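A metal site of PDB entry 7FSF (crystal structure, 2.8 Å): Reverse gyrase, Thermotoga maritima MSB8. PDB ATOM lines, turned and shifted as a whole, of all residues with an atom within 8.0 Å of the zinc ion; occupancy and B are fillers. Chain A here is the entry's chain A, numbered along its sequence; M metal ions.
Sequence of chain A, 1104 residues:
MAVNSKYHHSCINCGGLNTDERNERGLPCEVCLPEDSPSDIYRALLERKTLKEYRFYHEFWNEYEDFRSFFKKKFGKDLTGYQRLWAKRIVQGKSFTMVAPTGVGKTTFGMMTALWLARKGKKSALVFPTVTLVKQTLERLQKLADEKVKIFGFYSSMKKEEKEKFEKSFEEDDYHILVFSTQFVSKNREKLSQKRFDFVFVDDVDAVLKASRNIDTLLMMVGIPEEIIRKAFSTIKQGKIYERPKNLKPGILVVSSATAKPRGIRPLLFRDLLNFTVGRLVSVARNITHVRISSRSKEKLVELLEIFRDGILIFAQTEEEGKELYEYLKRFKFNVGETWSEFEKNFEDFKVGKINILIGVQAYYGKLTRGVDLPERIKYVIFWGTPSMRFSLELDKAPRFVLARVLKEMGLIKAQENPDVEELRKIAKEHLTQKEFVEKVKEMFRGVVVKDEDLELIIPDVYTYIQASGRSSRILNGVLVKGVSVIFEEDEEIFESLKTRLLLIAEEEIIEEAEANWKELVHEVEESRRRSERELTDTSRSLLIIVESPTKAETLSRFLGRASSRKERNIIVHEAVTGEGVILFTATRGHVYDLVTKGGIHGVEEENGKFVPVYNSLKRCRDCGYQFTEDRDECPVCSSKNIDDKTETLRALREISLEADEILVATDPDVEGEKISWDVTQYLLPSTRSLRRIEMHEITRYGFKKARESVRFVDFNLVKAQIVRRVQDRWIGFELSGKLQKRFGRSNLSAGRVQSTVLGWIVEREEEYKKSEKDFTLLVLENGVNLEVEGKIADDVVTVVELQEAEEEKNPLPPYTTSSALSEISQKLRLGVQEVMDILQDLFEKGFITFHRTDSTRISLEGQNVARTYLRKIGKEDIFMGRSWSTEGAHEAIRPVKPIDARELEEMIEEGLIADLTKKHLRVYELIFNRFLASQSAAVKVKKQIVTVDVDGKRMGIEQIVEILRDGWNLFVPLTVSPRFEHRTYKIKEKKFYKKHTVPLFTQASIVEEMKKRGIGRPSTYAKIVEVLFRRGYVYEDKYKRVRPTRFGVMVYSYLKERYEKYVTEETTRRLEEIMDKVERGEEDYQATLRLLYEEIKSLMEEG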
ATOM      1  N   ARG A 620      -2.348 -22.757  28.624  1.00  0.00           N
ATOM      2  CA  ARG A 620      -1.764 -21.676  29.404  1.00  0.00           C
ATOM      3  C   ARG A 620      -0.248 -21.856  29.417  1.00  0.00           C
ATOM      4  O   ARG A 620       0.253 -22.907  29.825  1.00  0.00           O
ATOM      5  CB  ARG A 620      -2.294 -21.691  30.841  1.00  0.00           C
ATOM      6  CG  ARG A 620      -3.790 -21.491  30.987  1.00  0.00           C
ATOM      7  CD  ARG A 620      -4.280 -22.025  32.331  1.00  0.00           C
ATOM      8  NE  ARG A 620      -5.595 -21.520  32.695  1.00  0.00           N
ATOM      9  CZ  ARG A 620      -6.735 -22.026  32.263  1.00  0.00           C
ATOM     10  NH1 ARG A 620      -6.773 -23.045  31.425  1.00  0.00           N
ATOM     11  NH2 ARG A 620      -7.880 -21.481  32.670  1.00  0.00           N
ATOM     12  N   CYS A 621       0.473 -20.826  28.968  1.00  0.00           N
ATOM     13  CA  CYS A 621       1.919 -20.833  29.103  1.00  0.00           C
ATOM     14  C   CYS A 621       2.292 -20.506  30.549  1.00  0.00           C
ATOM     15  O   CYS A 621       1.998 -19.416  31.040  1.00  0.00           O
ATOM     16  CB  CYS A 621       2.558 -19.822  28.145  1.00  0.00           C
ATOM     17  SG  CYS A 621       4.337 -19.632  28.362  1.00  0.00           S
ATOM     18  N   ARG A 622       2.925 -21.467  31.230  1.00  0.00           N
ATOM     19  CA  ARG A 622       3.189 -21.292  32.661  1.00  0.00           C
ATOM     20  C   ARG A 622       4.241 -20.229  32.936  1.00  0.00           C
ATOM     21  O   ARG A 622       4.365 -19.782  34.080  1.00  0.00           O
ATOM     22  CB  ARG A 622       3.625 -22.625  33.277  1.00  0.00           C
ATOM     23  CG  ARG A 622       2.574 -23.735  33.193  1.00  0.00           C
ATOM     24  CD  ARG A 622       2.916 -24.893  34.126  1.00  0.00           C
ATOM     25  NE  ARG A 622       2.183 -26.104  33.782  1.00  0.00           N
ATOM     26  CZ  ARG A 622       2.663 -27.071  33.010  1.00  0.00           C
ATOM     27  NH1 ARG A 622       3.870 -26.993  32.472  1.00  0.00           N
ATOM     28  NH2 ARG A 622       1.902 -28.142  32.764  1.00  0.00           N
ATOM     29  N   ASP A 623       4.988 -19.801  31.919  1.00  0.00           N
ATOM     30  CA  ASP A 623       6.080 -18.845  32.107  1.00  0.00           C
ATOM     31  C   ASP A 623       5.605 -17.405  31.932  1.00  0.00           C
ATOM     32  O   ASP A 623       5.749 -16.579  32.853  1.00  0.00           O
ATOM     33  CB  ASP A 623       7.218 -19.180  31.145  1.00  0.00           C
ATOM     34  CG  ASP A 623       7.785 -20.569  31.364  1.00  0.00           C
ATOM     35  OD1 ASP A 623       7.443 -21.184  32.396  1.00  0.00           O
ATOM     36  OD2 ASP A 623       8.568 -21.042  30.518  1.00  0.00           O
ATOM     37  N   CYS A 624       5.046 -17.074  30.771  1.00  0.00           N
ATOM     38  CA  CYS A 624       4.573 -15.725  30.502  1.00  0.00           C
ATOM     39  C   CYS A 624       3.081 -15.544  30.739  1.00  0.00           C
ATOM     40  O   CYS A 624       2.599 -14.409  30.738  1.00  0.00           O
ATOM     41  CB  CYS A 624       4.923 -15.303  29.067  1.00  0.00           C
ATOM     42  SG  CYS A 624       3.875 -16.004  27.767  1.00  0.00           S
ATOM     43  N   GLY A 625       2.337 -16.636  30.946  1.00  0.00           N
ATOM     44  CA  GLY A 625       0.926 -16.553  31.244  1.00  0.00           C
ATOM     45  C   GLY A 625       0.000 -16.495  30.044  1.00  0.00           C
ATOM     46  O   GLY A 625      -1.222 -16.498  30.230  1.00  0.00           O
ATOM     47  N   TYR A 626       0.544 -16.431  28.824  1.00  0.00           N
ATOM     48  CA  TYR A 626      -0.305 -16.276  27.657  1.00  0.00           C
ATOM     49  C   TYR A 626      -1.165 -17.512  27.454  1.00  0.00           C
ATOM     50  O   TYR A 626      -0.688 -18.647  27.522  1.00  0.00           O
ATOM     51  CB  TYR A 626       0.540 -16.015  26.404  1.00  0.00           C
ATOM     52  CG  TYR A 626      -0.304 -15.736  25.177  1.00  0.00           C
ATOM     53  CD1 TYR A 626      -1.171 -14.663  25.141  1.00  0.00           C
ATOM     54  CD2 TYR A 626      -0.232 -16.564  24.061  1.00  0.00           C
ATOM     55  CE1 TYR A 626      -1.948 -14.396  24.027  1.00  0.00           C
ATOM     56  CE2 TYR A 626      -1.004 -16.314  22.938  1.00  0.00           C
ATOM     57  CZ  TYR A 626      -1.860 -15.232  22.936  1.00  0.00           C
ATOM     58  OH  TYR A 626      -2.625 -14.970  21.817  1.00  0.00           O
ATOM     59  N   GLN A 627      -2.454 -17.284  27.197  1.00  0.00           N
ATOM     60  CA  GLN A 627      -3.400 -18.354  26.906  1.00  0.00           C
ATOM     61  C   GLN A 627      -3.693 -18.367  25.406  1.00  0.00           C
ATOM     62  O   GLN A 627      -3.956 -17.318  24.818  1.00  0.00           O
ATOM     63  CB  GLN A 627      -4.690 -18.179  27.702  1.00  0.00           C
ATOM     64  CG  GLN A 627      -4.477 -18.147  29.207  1.00  0.00           C
ATOM     65  CD  GLN A 627      -5.717 -18.532  29.980  1.00  0.00           C
ATOM     66  OE1 GLN A 627      -6.678 -19.042  29.404  1.00  0.00           O
ATOM     67  NE2 GLN A 627      -5.693 -18.309  31.286  1.00  0.00           N
ATOM     68  N   PHE A 628      -3.612 -19.547  24.806  1.00  0.00           N
ATOM     69  CA  PHE A 628      -3.853 -19.695  23.381  1.00  0.00           C
ATOM     70  C   PHE A 628      -4.623 -20.987  23.133  1.00  0.00           C
ATOM     71  O   PHE A 628      -4.641 -21.893  23.967  1.00  0.00           O
ATOM     72  CB  PHE A 628      -2.547 -19.667  22.577  1.00  0.00           C
ATOM     73  CG  PHE A 628      -1.526 -20.681  23.012  1.00  0.00           C
ATOM     74  CD1 PHE A 628      -0.713 -20.435  24.110  1.00  0.00           C
ATOM     75  CD2 PHE A 628      -1.354 -21.847  22.296  1.00  0.00           C
ATOM     76  CE1 PHE A 628       0.231 -21.359  24.501  1.00  0.00           C
ATOM     77  CE2 PHE A 628      -0.406 -22.784  22.692  1.00  0.00           C
ATOM     78  CZ  PHE A 628       0.386 -22.535  23.796  1.00  0.00           C
ATOM     79  N   GLU A 634       5.483 -24.858  20.834  1.00  0.00           N
ATOM     80  CA  GLU A 634       6.061 -23.760  21.600  1.00  0.00           C
ATOM     81  C   GLU A 634       5.028 -22.662  21.813  1.00  0.00           C
ATOM     82  O   GLU A 634       4.094 -22.502  21.012  1.00  0.00           O
ATOM     83  CB  GLU A 634       7.290 -23.202  20.891  1.00  0.00           C
ATOM     84  CG  GLU A 634       8.401 -24.217  20.695  1.00  0.00           C
ATOM     85  CD  GLU A 634       9.645 -23.624  20.041  1.00  0.00           C
ATOM     86  OE1 GLU A 634       9.504 -22.885  19.052  1.00  0.00           O
ATOM     87  OE2 GLU A 634      10.759 -23.895  20.543  1.00  0.00           O
ATOM     88  N   CYS A 635       5.207 -21.900  22.887  1.00  0.00           N
ATOM     89  CA  CYS A 635       4.330 -20.775  23.163  1.00  0.00           C
ATOM     90  C   CYS A 635       4.454 -19.726  22.053  1.00  0.00           C
ATOM     91  O   CYS A 635       5.583 -19.378  21.668  1.00  0.00           O
ATOM     92  CB  CYS A 635       4.663 -20.138  24.515  1.00  0.00           C
ATOM     93  SG  CYS A 635       3.861 -18.536  24.828  1.00  0.00           S
ATOM     94  N   PRO A 636       3.350 -19.210  21.529  1.00  0.00           N
ATOM     95  CA  PRO A 636       3.453 -18.216  20.446  1.00  0.00           C
ATOM     96  C   PRO A 636       4.129 -16.914  20.853  1.00  0.00           C
ATOM     97  O   PRO A 636       4.500 -16.124  19.976  1.00  0.00           O
ATOM     98  CB  PRO A 636       1.987 -17.972  20.049  1.00  0.00           C
ATOM     99  CG  PRO A 636       1.188 -18.423  21.223  1.00  0.00           C
ATOM    100  CD  PRO A 636       1.957 -19.547  21.848  1.00  0.00           C
ATOM    101  N   VAL A 637       4.287 -16.655  22.143  1.00  0.00           N
ATOM    102  CA  VAL A 637       4.845 -15.374  22.569  1.00  0.00           C
ATOM    103  C   VAL A 637       6.317 -15.523  22.916  1.00  0.00           C
ATOM    104  O   VAL A 637       7.164 -14.793  22.380  1.00  0.00           O
ATOM    105  CB  VAL A 637       4.065 -14.811  23.775  1.00  0.00           C
ATOM    106  CG1 VAL A 637       4.740 -13.567  24.302  1.00  0.00           C
ATOM    107  CG2 VAL A 637       2.634 -14.489  23.357  1.00  0.00           C
ATOM    108  N   CYS A 638       6.642 -16.452  23.816  1.00  0.00           N
ATOM    109  CA  CYS A 638       8.012 -16.607  24.306  1.00  0.00           C
ATOM    110  C   CYS A 638       8.647 -17.928  23.905  1.00  0.00           C
ATOM    111  O   CYS A 638       9.726 -18.249  24.416  1.00  0.00           O
ATOM    112  CB  CYS A 638       8.037 -16.454  25.827  1.00  0.00           C
ATOM    113  SG  CYS A 638       7.049 -17.673  26.715  1.00  0.00           S
ATOM    114  N   SER A 639       8.024 -18.704  23.018  1.00  0.00           N
ATOM    115  CA  SER A 639       8.583 -19.959  22.507  1.00  0.00           C
ATOM    116  C   SER A 639       8.982 -20.918  23.632  1.00  0.00           C
ATOM    117  O   SER A 639      10.011 -21.588  23.577  1.00  0.00           O
ATOM    118  CB  SER A 639       9.788 -19.698  21.591  1.00  0.00           C
ATOM    119  OG  SER A 639       9.375 -19.197  20.334  1.00  0.00           O
ATOM    120  N   SER A 640       8.146 -20.983  24.677  1.00  0.00           N
ATOM    121  CA  SER A 640       8.365 -21.880  25.803  1.00  0.00           C
ATOM    122  C   SER A 640       7.537 -23.138  25.638  1.00  0.00           C
ATOM    123  O   SER A 640       6.359 -23.078  25.274  1.00  0.00           O
ATOM    124  CB  SER A 640       8.018 -21.188  27.126  1.00  0.00           C
ATOM    125  OG  SER A 640       8.111 -22.102  28.209  1.00  0.00           O
ATOM    126  N   LYS A 641       8.156 -24.290  25.922  1.00  0.00           N
ATOM    127  CA  LYS A 641       7.490 -25.588  25.868  1.00  0.00           C
ATOM    128  C   LYS A 641       7.008 -26.043  27.244  1.00  0.00           C
ATOM    129  O   LYS A 641       7.001 -27.253  27.528  1.00  0.00           O
ATOM    130  CB  LYS A 641       8.413 -26.632  25.239  1.00  0.00           C
ATOM    131  CG  LYS A 641       8.678 -26.410  23.761  1.00  0.00           C
ATOM    132  CD  LYS A 641       9.396 -27.599  23.141  1.00  0.00           C
ATOM    133  CE  LYS A 641       9.259 -27.577  21.619  1.00  0.00           C
ATOM    134  NZ  LYS A 641       9.890 -28.763  20.987  1.00  0.00           N
ATOM    135  N   ASN A 642       6.608 -25.103  28.096  1.00  0.00           N
ATOM    136  CA  ASN A 642       6.168 -25.407  29.447  1.00  0.00           C
ATOM    137  C   ASN A 642       4.698 -25.060  29.615  1.00  0.00           C
ATOM    138  O   ASN A 642       4.296 -24.475  30.629  1.00  0.00           O
ATOM    139  CB  ASN A 642       7.031 -24.644  30.461  1.00  0.00           C
ATOM    140  CG  ASN A 642       6.874 -25.171  31.874  1.00  0.00           C
ATOM    141  OD1 ASN A 642       6.831 -26.386  32.098  1.00  0.00           O
ATOM    142  ND2 ASN A 642       6.787 -24.277  32.844  1.00  0.00           N
ATOM    143  N   ILE A 643       3.885 -25.402  28.620  1.00  0.00           N
ATOM    144  CA  ILE A 643       2.499 -24.957  28.566  1.00  0.00           C
ATOM    145  C   ILE A 643       1.607 -25.933  29.321  1.00  0.00           C
ATOM    146  O   ILE A 643       1.840 -27.149  29.313  1.00  0.00           O
ATOM    147  CB  ILE A 643       2.033 -24.796  27.101  1.00  0.00           C
ATOM    148  CG1 ILE A 643       2.041 -26.141  26.371  1.00  0.00           C
ATOM    149  CG2 ILE A 643       2.938 -23.824  26.363  1.00  0.00           C
ATOM    150  CD1 ILE A 643       1.547 -26.041  24.943  1.00  0.00           C
HETATM  151 ZN    ZN M   1       4.774 -17.884  26.904  1.00  0.00          ZN
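The zinc ion is bound by SG of Cys 624 (2.3 Å), SG of Cys 638 (2.3 Å), SG of Cys 621 (2.3 Å) and SG of Cys 635 (2.4 Å).
SG of Cys 621 sits close to N of Asp 623.
N of Cys 621 is in hydrogen-bond range of O of Tyr 626, at 2.9 Å.
The backbone NH (N) of Cys 635 sits at hydrogen-bond distance from the backbone carbonyl oxygen (O) of Ser 640 (2.9 Å).
The side-chain sulfur (SG) of Cys 624 lies close to the backbone NH (N) of Tyr 626, 3.5 Å away.
The backbone NH of Val 637 sits close to the side-chain sulfur of Cys 635, at 3.3 Å.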
